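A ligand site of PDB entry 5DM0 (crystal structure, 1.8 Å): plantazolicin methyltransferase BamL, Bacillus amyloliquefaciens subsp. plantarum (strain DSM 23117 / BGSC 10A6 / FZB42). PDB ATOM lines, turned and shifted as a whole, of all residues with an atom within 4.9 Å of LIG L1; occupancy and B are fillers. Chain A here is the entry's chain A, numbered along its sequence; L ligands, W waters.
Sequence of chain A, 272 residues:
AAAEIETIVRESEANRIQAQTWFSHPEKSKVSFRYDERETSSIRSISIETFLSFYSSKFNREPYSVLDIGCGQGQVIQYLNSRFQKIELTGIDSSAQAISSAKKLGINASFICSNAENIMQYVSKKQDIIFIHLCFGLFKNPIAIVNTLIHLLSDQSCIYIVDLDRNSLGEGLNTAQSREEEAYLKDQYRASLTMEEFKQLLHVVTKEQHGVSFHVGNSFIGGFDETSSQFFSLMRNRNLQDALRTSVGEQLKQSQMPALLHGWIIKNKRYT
OD2 of Asp 36 sits close to S1 of LIG L1, at 3.7 Å. CE1 of Phe 23 touches S1 of LIG L1, 3.5 Å away. Gly 72 touches LIG L1. Ser 95 touches LIG L1. Ser 114 touches LIG L1. Leu 134 touches LIG L1 (O to C2, 3.9 Å). CB of Cys 135 touches O3 of LIG L1 (3.6 Å). CD1 of Leu 138 touches C5 of LIG L1 (3.6 Å). Phe 139 touches LIG L1. Within 4 Å of LIG L1: Gln 20, Phe 23, Asp 36, Gly 70, Gly 72, Asp 93, Ser 94, Ser 95, Ser 114, Asn 115, Ala 116, His 133, Leu 134, Cys 135, Leu 138 and Phe 139. The nearest printed residue that does not touch LIG L1 is Ile 92 (4.2 Å).
A nitrogen (N4) of LG2 L2 lies close to a sulfur (S1) of LIG L1 (3.4 Å).
O5 of LIG L1 lies within hydrogen-bond range of OD1 of Asp 93, 2.5 Å away. N1 of LIG L1 lies within hydrogen-bond range of O of Gly 70. The backbone carbonyl oxygen (O) of His 133 is in hydrogen-bond range of a nitrogen (N1) of LIG L1. The backbone NH of Ala 116 lies within hydrogen-bond range of a nitrogen (N5) of LIG L1, at 2.9 Å. A nitrogen (N4) of LIG L1 sits at hydrogen-bond distance from the side-chain amide oxygen (OD1) of Asn 115, 2.9 Å away. The side-chain amide oxygen of Gln 20 sits close to a nitrogen (N3) of LIG L1 (3.5 Å). N6 of LIG L1 lies within hydrogen-bond range of N of Ser 94, 3.3 Å away. A nitrogen (N4) of LG2 L2 is in salt-bridge range of the side-chain carboxylate (OD2) of Asp 36, at 3.6 Å. The backbone carbonyl oxygen of Leu 134 lies within hydrogen-bond range of a nitrogen (N4) of LG2 L2, at 2.9 Å.
The backbone NH (N) of Ser 95 is in hydrogen-bond range of the side-chain carboxylate (OD1) of Asp 93, 2.9 Å away. N of Gly 72 lies within hydrogen-bond range of OD2 of Asp 93 (2.8 Å). The backbone carbonyl oxygen (O) of Asp 93 lies within hydrogen-bond range of the backbone NH (N) of Ser 114 (3.1 Å). N of Gly 70 is in hydrogen-bond range of O of Ile 92. The backbone NH (N) of Ser 94 is in hydrogen-bond range of the backbone carbonyl oxygen (O) of Ser 114 (3.4 Å). The side-chain hydroxyl (OG) of Ser 95 is in hydrogen-bond range of the backbone NH (N) of Ala 98. The side-chain sulfur (SG) of Cys 135 is in hydrogen-bond range of the backbone carbonyl oxygen (O) of Ile 69. The side-chain hydroxyl (OG1) of Thr 40 is in hydrogen-bond range of the backbone carbonyl oxygen (O) of Asp 36 (2.6 Å).
Water W4 lies within hydrogen-bond range of a nitrogen (N3) of LIG L1 (2.7 Å) and the backbone carbonyl oxygen (O) of Leu 138 (2.8 Å). Water W5 lies within hydrogen-bond range of a nitrogen (N1) of LIG L1 (2.7 Å) and the side-chain carboxylate of Asp 68 (2.8 Å). Water W2 lies within hydrogen-bond range of an oxygen (O5) of LIG L1 (2.7 Å), the side-chain hydroxyl of Ser 94 (2.8 Å) and the side-chain amide nitrogen of Gln 20 (3.0 Å). Water W1 lies within hydrogen-bond range of a nitrogen (N4) of LG2 L2, the side-chain hydroxyl of Thr 40 and an oxygen (O1) of LIG L1. Water W3 lies within hydrogen-bond range of the backbone carbonyl oxygen (O) of Ile 69 (2.6 Å), the side-chain carboxylate (OD1) of Asp 68 (2.7 Å), the backbone NH (N) of His 133 (2.7 Å) and a nitrogen (N1) of LIG L1 (3.1 Å). Water W6 lies within hydrogen-bond range of the side-chain hydroxyl (OG) of Ser 94, the side-chain amide nitrogen (NE2) of Gln 20 and a nitrogen (N4) of LIG L1.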
ATOM      1  N   GLN A  20      13.696 -13.586  11.621  1.00  0.00           N
ATOM      2  CA  GLN A  20      13.877 -14.954  11.122  1.00  0.00           C
ATOM      3  C   GLN A  20      15.093 -15.651  11.727  1.00  0.00           C
ATOM      4  O   GLN A  20      15.099 -16.889  11.810  1.00  0.00           O
ATOM      5  CB  GLN A  20      13.889 -14.979   9.577  1.00  0.00           C
ATOM      6  CG  GLN A  20      14.305 -16.292   8.917  1.00  0.00           C
ATOM      7  CD  GLN A  20      13.444 -17.505   9.269  1.00  0.00           C
ATOM      8  OE1 GLN A  20      12.399 -17.398   9.926  1.00  0.00           O
ATOM      9  NE2 GLN A  20      13.896 -18.681   8.845  1.00  0.00           N
ATOM     10  N   PHE A  23      14.594 -18.494  14.090  1.00  0.00           N
ATOM     11  CA  PHE A  23      14.182 -19.807  13.599  1.00  0.00           C
ATOM     12  C   PHE A  23      15.285 -20.509  12.814  1.00  0.00           C
ATOM     13  O   PHE A  23      15.159 -21.682  12.498  1.00  0.00           O
ATOM     14  CB  PHE A  23      12.903 -19.672  12.774  1.00  0.00           C
ATOM     15  CG  PHE A  23      11.746 -19.199  13.602  1.00  0.00           C
ATOM     16  CD1 PHE A  23      11.040 -20.102  14.387  1.00  0.00           C
ATOM     17  CD2 PHE A  23      11.441 -17.845  13.671  1.00  0.00           C
ATOM     18  CE1 PHE A  23      10.004 -19.663  15.206  1.00  0.00           C
ATOM     19  CE2 PHE A  23      10.416 -17.393  14.492  1.00  0.00           C
ATOM     20  CZ  PHE A  23       9.702 -18.310  15.260  1.00  0.00           C
ATOM     21  N   ASP A  36       6.862 -20.425  21.679  1.00  0.00           N
ATOM     22  CA  ASP A  36       5.725 -20.731  20.791  1.00  0.00           C
ATOM     23  C   ASP A  36       4.856 -21.872  21.313  1.00  0.00           C
ATOM     24  O   ASP A  36       3.636 -21.767  21.347  1.00  0.00           O
ATOM     25  CB  ASP A  36       6.228 -21.020  19.371  1.00  0.00           C
ATOM     26  CG  ASP A  36       6.886 -19.813  18.715  1.00  0.00           C
ATOM     27  OD1 ASP A  36       6.921 -18.724  19.324  1.00  0.00           O
ATOM     28  OD2 ASP A  36       7.395 -19.955  17.575  1.00  0.00           O
ATOM     29  N   THR A  40       1.495 -20.047  22.238  1.00  0.00           N
ATOM     30  CA  THR A  40       0.763 -19.938  20.966  1.00  0.00           C
ATOM     31  C   THR A  40      -0.057 -21.188  20.583  1.00  0.00           C
ATOM     32  O   THR A  40      -0.775 -21.181  19.576  1.00  0.00           O
ATOM     33  CB  THR A  40       1.670 -19.488  19.792  1.00  0.00           C
ATOM     34  OG1 THR A  40       2.447 -20.598  19.321  1.00  0.00           O
ATOM     35  CG2 THR A  40       2.615 -18.372  20.241  1.00  0.00           C
ATOM     36  N   ASP A  68      -0.365 -25.700   4.337  1.00  0.00           N
ATOM     37  CA  ASP A  68       0.040 -25.000   5.560  1.00  0.00           C
ATOM     38  C   ASP A  68       1.436 -24.405   5.385  1.00  0.00           C
ATOM     39  O   ASP A  68       2.428 -25.133   5.249  1.00  0.00           O
ATOM     40  CB  ASP A  68      -0.020 -25.965   6.752  1.00  0.00           C
ATOM     41  CG  ASP A  68       0.123 -25.259   8.100  1.00  0.00           C
ATOM     42  OD1 ASP A  68      -0.216 -24.058   8.207  1.00  0.00           O
ATOM     43  OD2 ASP A  68       0.579 -25.914   9.055  1.00  0.00           O
ATOM     44  N   ILE A  69       1.485 -23.073   5.327  1.00  0.00           N
ATOM     45  CA  ILE A  69       2.714 -22.319   5.098  1.00  0.00           C
ATOM     46  C   ILE A  69       3.426 -22.020   6.423  1.00  0.00           C
ATOM     47  O   ILE A  69       2.817 -21.434   7.338  1.00  0.00           O
ATOM     48  CB  ILE A  69       2.395 -20.975   4.368  1.00  0.00           C
ATOM     49  CG1 ILE A  69       1.604 -21.201   3.061  1.00  0.00           C
ATOM     50  CG2 ILE A  69       3.659 -20.139   4.160  1.00  0.00           C
ATOM     51  CD1 ILE A  69       2.295 -21.987   1.957  1.00  0.00           C
ATOM     52  N   GLY A  70       4.700 -22.416   6.522  1.00  0.00           N
ATOM     53  CA  GLY A  70       5.471 -22.302   7.770  1.00  0.00           C
ATOM     54  C   GLY A  70       4.864 -23.251   8.786  1.00  0.00           C
ATOM     55  O   GLY A  70       4.520 -22.843   9.913  1.00  0.00           O
ATOM     56  N   CYS A  71       4.742 -24.524   8.401  1.00  0.00           N
ATOM     57  CA  CYS A  71       3.967 -25.520   9.129  1.00  0.00           C
ATOM     58  C   CYS A  71       4.589 -26.001  10.442  1.00  0.00           C
ATOM     59  O   CYS A  71       3.967 -26.764  11.192  1.00  0.00           O
ATOM     60  CB  CYS A  71       3.686 -26.724   8.224  1.00  0.00           C
ATOM     61  SG  CYS A  71       5.184 -27.625   7.758  1.00  0.00           S
ATOM     62  N   GLY A  72       5.822 -25.569  10.705  1.00  0.00           N
ATOM     63  CA  GLY A  72       6.538 -25.939  11.928  1.00  0.00           C
ATOM     64  C   GLY A  72       6.655 -27.451  12.032  1.00  0.00           C
ATOM     65  O   GLY A  72       6.979 -28.136  11.059  1.00  0.00           O
ATOM     66  N   VAL A  76      -0.496 -28.297  13.072  1.00  0.00           N
ATOM     67  CA  VAL A  76      -1.748 -27.944  12.371  1.00  0.00           C
ATOM     68  C   VAL A  76      -2.228 -29.078  11.473  1.00  0.00           C
ATOM     69  O   VAL A  76      -3.400 -29.447  11.482  1.00  0.00           O
ATOM     70  CB  VAL A  76      -1.604 -26.620  11.582  1.00  0.00           C
ATOM     71  CG1 VAL A  76      -2.762 -26.446  10.600  1.00  0.00           C
ATOM     72  CG2 VAL A  76      -1.522 -25.444  12.539  1.00  0.00           C
ATOM     73  N   ILE A  92       4.664 -26.820   4.363  1.00  0.00           N
ATOM     74  CA  ILE A  92       5.995 -26.388   3.930  1.00  0.00           C
ATOM     75  C   ILE A  92       6.642 -25.521   5.022  1.00  0.00           C
ATOM     76  O   ILE A  92       5.999 -24.652   5.613  1.00  0.00           O
ATOM     77  CB  ILE A  92       5.968 -25.655   2.551  1.00  0.00           C
ATOM     78  CG1 ILE A  92       7.392 -25.276   2.096  1.00  0.00           C
ATOM     79  CG2 ILE A  92       5.072 -24.425   2.583  1.00  0.00           C
ATOM     80  CD1 ILE A  92       7.542 -25.066   0.599  1.00  0.00           C
ATOM     81  N   ASP A  93       7.927 -25.769   5.287  1.00  0.00           N
ATOM     82  CA  ASP A  93       8.677 -25.004   6.279  1.00  0.00           C
ATOM     83  C   ASP A  93      10.150 -25.042   5.915  1.00  0.00           C
ATOM     84  O   ASP A  93      10.646 -26.059   5.461  1.00  0.00           O
ATOM     85  CB  ASP A  93       8.476 -25.592   7.686  1.00  0.00           C
ATOM     86  CG  ASP A  93       8.816 -24.608   8.782  1.00  0.00           C
ATOM     87  OD1 ASP A  93      10.020 -24.314   8.968  1.00  0.00           O
ATOM     88  OD2 ASP A  93       7.882 -24.108   9.447  1.00  0.00           O
ATOM     89  N   SER A  94      10.853 -23.936   6.102  1.00  0.00           N
ATOM     90  CA  SER A  94      12.266 -23.875   5.730  1.00  0.00           C
ATOM     91  C   SER A  94      13.222 -24.440   6.792  1.00  0.00           C
ATOM     92  O   SER A  94      14.438 -24.488   6.568  1.00  0.00           O
ATOM     93  CB  SER A  94      12.661 -22.457   5.304  1.00  0.00           C
ATOM     94  OG  SER A  94      12.385 -21.508   6.326  1.00  0.00           O
ATOM     95  N   SER A  95      12.674 -24.863   7.934  1.00  0.00           N
ATOM     96  CA  SER A  95      13.493 -25.478   8.988  1.00  0.00           C
ATOM     97  C   SER A  95      13.555 -26.991   8.827  1.00  0.00           C
ATOM     98  O   SER A  95      12.543 -27.683   8.985  1.00  0.00           O
ATOM     99  CB  SER A  95      12.980 -25.131  10.391  1.00  0.00           C
ATOM    100  OG  SER A  95      13.559 -25.984  11.391  1.00  0.00           O
ATOM    101  N   ALA A  98      12.362 -28.790  11.911  1.00  0.00           N
ATOM    102  CA  ALA A  98      10.911 -28.768  12.020  1.00  0.00           C
ATOM    103  C   ALA A  98      10.290 -29.845  11.133  1.00  0.00           C
ATOM    104  O   ALA A  98       9.426 -30.603  11.578  1.00  0.00           O
ATOM    105  CB  ALA A  98      10.352 -27.386  11.657  1.00  0.00           C
ATOM    106  N   SER A 114      11.521 -26.275   2.492  1.00  0.00           N
ATOM    107  CA  SER A 114      11.985 -25.268   1.545  1.00  0.00           C
ATOM    108  C   SER A 114      11.428 -23.932   2.009  1.00  0.00           C
ATOM    109  O   SER A 114      10.457 -23.897   2.762  1.00  0.00           O
ATOM    110  CB  SER A 114      11.464 -25.578   0.138  1.00  0.00           C
ATOM    111  OG  SER A 114      12.196 -24.869  -0.862  1.00  0.00           O
ATOM    112  N   ASN A 115      12.060 -22.837   1.566  1.00  0.00           N
ATOM    113  CA  ASN A 115      11.423 -21.512   1.586  1.00  0.00           C
ATOM    114  C   ASN A 115      10.061 -21.610   0.892  1.00  0.00           C
ATOM    115  O   ASN A 115       9.955 -22.186  -0.183  1.00  0.00           O
ATOM    116  CB  ASN A 115      12.299 -20.513   0.822  1.00  0.00           C
ATOM    117  CG  ASN A 115      11.959 -19.071   1.141  1.00  0.00           C
ATOM    118  OD1 ASN A 115      10.781 -18.672   1.222  1.00  0.00           O
ATOM    119  ND2 ASN A 115      12.997 -18.256   1.304  1.00  0.00           N
ATOM    120  N   ALA A 116       9.028 -21.043   1.521  1.00  0.00           N
ATOM    121  CA  ALA A 116       7.694 -21.059   0.932  1.00  0.00           C
ATOM    122  C   ALA A 116       7.640 -20.309  -0.410  1.00  0.00           C
ATOM    123  O   ALA A 116       6.751 -20.569  -1.231  1.00  0.00           O
ATOM    124  CB  ALA A 116       6.656 -20.506   1.907  1.00  0.00           C
ATOM    125  N   HIS A 133      -0.095 -19.155   9.356  1.00  0.00           N
ATOM    126  CA  HIS A 133      -0.356 -18.912  10.778  1.00  0.00           C
ATOM    127  C   HIS A 133       0.910 -18.521  11.533  1.00  0.00           C
ATOM    128  O   HIS A 133       1.871 -19.303  11.609  1.00  0.00           O
ATOM    129  CB  HIS A 133      -0.989 -20.178  11.382  1.00  0.00           C
ATOM    130  CG  HIS A 133      -1.556 -20.017  12.755  1.00  0.00           C
ATOM    131  ND1 HIS A 133      -2.683 -19.261  13.006  1.00  0.00           N
ATOM    132  CD2 HIS A 133      -1.202 -20.570  13.941  1.00  0.00           C
ATOM    133  CE1 HIS A 133      -2.969 -19.328  14.299  1.00  0.00           C
ATOM    134  NE2 HIS A 133      -2.099 -20.125  14.883  1.00  0.00           N
ATOM    135  N   LEU A 134       0.908 -17.299  12.088  1.00  0.00           N
ATOM    136  CA  LEU A 134       1.970 -16.787  12.942  1.00  0.00           C
ATOM    137  C   LEU A 134       3.380 -16.868  12.327  1.00  0.00           C
ATOM    138  O   LEU A 134       4.345 -17.198  13.031  1.00  0.00           O
ATOM    139  CB  LEU A 134       1.940 -17.471  14.323  1.00  0.00           C
ATOM    140  CG  LEU A 134       0.555 -17.557  14.983  1.00  0.00           C
ATOM    141  CD1 LEU A 134       0.593 -18.376  16.265  1.00  0.00           C
ATOM    142  CD2 LEU A 134       0.009 -16.158  15.237  1.00  0.00           C
ATOM    143  N   CYS A 135       3.488 -16.540  11.034  1.00  0.00           N
ATOM    144  CA  CYS A 135       4.797 -16.539  10.353  1.00  0.00           C
ATOM    145  C   CYS A 135       4.999 -15.468   9.269  1.00  0.00           C
ATOM    146  O   CYS A 135       6.097 -15.339   8.721  1.00  0.00           O
ATOM    147  CB  CYS A 135       5.122 -17.929   9.790  1.00  0.00           C
ATOM    148  SG  CYS A 135       3.993 -18.511   8.497  1.00  0.00           S
ATOM    149  N   LEU A 138       7.989 -13.155   9.019  1.00  0.00           N
ATOM    150  CA  LEU A 138       9.316 -13.790   8.852  1.00  0.00           C
ATOM    151  C   LEU A 138       9.772 -13.811   7.395  1.00  0.00           C
ATOM    152  O   LEU A 138      10.944 -14.031   7.100  1.00  0.00           O
ATOM    153  CB  LEU A 138       9.312 -15.199   9.427  1.00  0.00           C
ATOM    154  CG  LEU A 138       8.956 -15.338  10.915  1.00  0.00           C
ATOM    155  CD1 LEU A 138       8.869 -16.809  11.272  1.00  0.00           C
ATOM    156  CD2 LEU A 138       9.952 -14.598  11.802  1.00  0.00           C
ATOM    157  N   PHE A 139       8.844 -13.583   6.469  1.00  0.00           N
ATOM    158  CA  PHE A 139       9.152 -13.660   5.053  1.00  0.00           C
ATOM    159  C   PHE A 139       9.935 -12.425   4.597  1.00  0.00           C
ATOM    160  O   PHE A 139       9.540 -11.290   4.882  1.00  0.00           O
ATOM    161  CB  PHE A 139       7.879 -13.802   4.213  1.00  0.00           C
ATOM    162  CG  PHE A 139       7.045 -14.997   4.592  1.00  0.00           C
ATOM    163  CD1 PHE A 139       7.623 -16.160   5.063  1.00  0.00           C
ATOM    164  CD2 PHE A 139       5.659 -14.945   4.461  1.00  0.00           C
ATOM    165  CE1 PHE A 139       6.837 -17.260   5.407  1.00  0.00           C
ATOM    166  CE2 PHE A 139       4.878 -16.030   4.792  1.00  0.00           C
ATOM    167  CZ  PHE A 139       5.458 -17.180   5.263  1.00  0.00           C
ATOM    168  N   ILE A 145       5.501 -13.633  -1.984  1.00  0.00           N
ATOM    169  CA  ILE A 145       4.965 -14.944  -1.567  1.00  0.00           C
ATOM    170  C   ILE A 145       3.431 -14.955  -1.707  1.00  0.00           C
ATOM    171  O   ILE A 145       2.852 -15.924  -2.210  1.00  0.00           O
ATOM    172  CB  ILE A 145       5.416 -15.366  -0.147  1.00  0.00           C
ATOM    173  CG1 ILE A 145       6.925 -15.629  -0.116  1.00  0.00           C
ATOM    174  CG2 ILE A 145       4.712 -16.645   0.305  1.00  0.00           C
ATOM    175  CD1 ILE A 145       7.490 -15.949   1.255  1.00  0.00           C
HETATM  176  N1  LIG L   1       2.565 -22.006  11.562  1.00  0.00           N
HETATM  177  C1  LIG L   1       3.324 -22.146  12.840  1.00  0.00           C
HETATM  178  C2  LIG L   1       4.383 -21.055  12.938  1.00  0.00           C
HETATM  179  C3  LIG L   1       5.609 -21.632  13.652  1.00  0.00           C
HETATM  180  S1  LIG L   1       6.838 -20.410  13.979  1.00  0.00           S
HETATM  181  C4  LIG L   1       2.349 -22.027  13.982  1.00  0.00           C
HETATM  182  O1  LIG L   1       2.716 -21.827  15.142  1.00  0.00           O
HETATM  183  O2  LIG L   1       1.144 -22.157  13.785  1.00  0.00           O
HETATM  184  C5  LIG L   1       7.239 -19.800  12.368  1.00  0.00           C
HETATM  185  C6  LIG L   1       7.634 -20.904  11.388  1.00  0.00           C
HETATM  186  O3  LIG L   1       7.841 -20.323  10.091  1.00  0.00           O
HETATM  187  C7  LIG L   1       8.955 -21.597  11.742  1.00  0.00           C
HETATM  188  O4  LIG L   1       8.739 -23.018  11.816  1.00  0.00           O
HETATM  189  C8  LIG L   1       9.914 -21.252  10.610  1.00  0.00           C
HETATM  190  O5  LIG L   1      10.828 -22.305  10.297  1.00  0.00           O
HETATM  191  C9  LIG L   1       8.945 -20.984   9.464  1.00  0.00           C
HETATM  192  N2  LIG L   1       9.453 -20.123   8.385  1.00  0.00           N
HETATM  193  C10 LIG L   1      10.105 -18.947   8.510  1.00  0.00           C
HETATM  194  N3  LIG L   1      10.382 -18.431   7.286  1.00  0.00           N
HETATM  195  C11 LIG L   1       9.913 -19.296   6.371  1.00  0.00           C
HETATM  196  C12 LIG L   1       9.875 -19.372   4.889  1.00  0.00           C
HETATM  197  N4  LIG L   1      10.419 -18.396   4.126  1.00  0.00           N
HETATM  198  N5  LIG L   1       9.281 -20.461   4.348  1.00  0.00           N
HETATM  199  C13 LIG L   1       8.741 -21.452   5.083  1.00  0.00           C
HETATM  200  N6  LIG L   1       8.728 -21.448   6.433  1.00  0.00           N
HETATM  201  C14 LIG L   1       9.298 -20.408   7.106  1.00  0.00           C
HETATM  202  C1  LG2 L   2       4.958 -14.603  19.311  1.00  0.00           C
HETATM  203  C2  LG2 L   2       3.915 -15.310  18.704  1.00  0.00           C
HETATM  204  C3  LG2 L   2       0.929 -15.049  20.519  1.00  0.00           C
HETATM  205  C4  LG2 L   2       5.440 -16.203  17.354  1.00  0.00           C
HETATM  206  C5  LG2 L   2       0.414 -15.695  19.300  1.00  0.00           C
HETATM  207  C6  LG2 L   2       2.522 -15.281  19.215  1.00  0.00           C
HETATM  208  C7  LG2 L   2       0.148 -14.808  21.729  1.00  0.00           C
HETATM  209  C8  LG2 L   2      -0.638 -14.493  24.043  1.00  0.00           C
HETATM  210  C9  LG2 L   2      -1.614 -14.786  23.088  1.00  0.00           C
HETATM  211  O1  LG2 L   2      -3.449 -14.394  24.489  1.00  0.00           O
HETATM  212  C10 LG2 L   2      -3.050 -14.894  23.448  1.00  0.00           C
HETATM  213  O2  LG2 L   2      -3.935 -15.638  22.564  1.00  0.00           O
HETATM  214  N1  LG2 L   2      -1.173 -14.991  21.804  1.00  0.00           N
HETATM  215  S1  LG2 L   2       0.884 -14.477  23.240  1.00  0.00           S
HETATM  216  N2  LG2 L   2       2.253 -14.866  20.474  1.00  0.00           N
HETATM  217  O3  LG2 L   2       1.497 -15.819  18.464  1.00  0.00           O
HETATM  218  C11 LG2 L   2      -0.931 -16.136  18.790  1.00  0.00           C
HETATM  219  S2  LG2 L   2       6.329 -15.112  18.384  1.00  0.00           S
HETATM  220  N3  LG2 L   2       4.142 -16.197  17.699  1.00  0.00           N
HETATM  221  C12 LG2 L   2       6.152 -16.977  16.299  1.00  0.00           C
HETATM  222  N4  LG2 L   2       5.206 -17.886  15.665  1.00  0.00           N
HETATM  223  C13 LG2 L   2       6.812 -16.075  15.251  1.00  0.00           C
HETATM  224  C14 LG2 L   2       5.901 -14.969  14.718  1.00  0.00           C
HETATM  225  C15 LG2 L   2       6.417 -14.556  13.338  1.00  0.00           C
HETATM  226  N5  LG2 L   2       5.684 -13.348  12.934  1.00  0.00           N
HETATM  227  C16 LG2 L   2       6.012 -12.139  13.148  1.00  0.00           C
HETATM  228  N6  LG2 L   2       5.263 -11.192  12.738  1.00  0.00           N
HETATM  229  N7  LG2 L   2       7.078 -11.847  13.782  1.00  0.00           N
HETATM  230  C17 LG2 L   2      -5.321 -15.772  22.870  1.00  0.00           C
HETATM  231  C18 LG2 L   2      -5.698 -17.240  22.904  1.00  0.00           C
HETATM  232  O   HOH W   1       3.874 -19.885  17.009  1.00  0.00           O
HETATM  233  O   HOH W   2      13.119 -21.544   9.008  1.00  0.00           O
HETATM  234  O   HOH W   3       0.797 -21.728   9.023  1.00  0.00           O
HETATM  235  O   HOH W   4      11.968 -16.502   6.302  1.00  0.00           O
HETATM  236  O   HOH W   5       1.094 -24.254  11.188  1.00  0.00           O
HETATM  237  O   HOH W   6      13.474 -19.237   5.526  1.00  0.00           O
HETATM  238  O   HOH W   7      10.602 -24.191  13.386  1.00  0.00           O
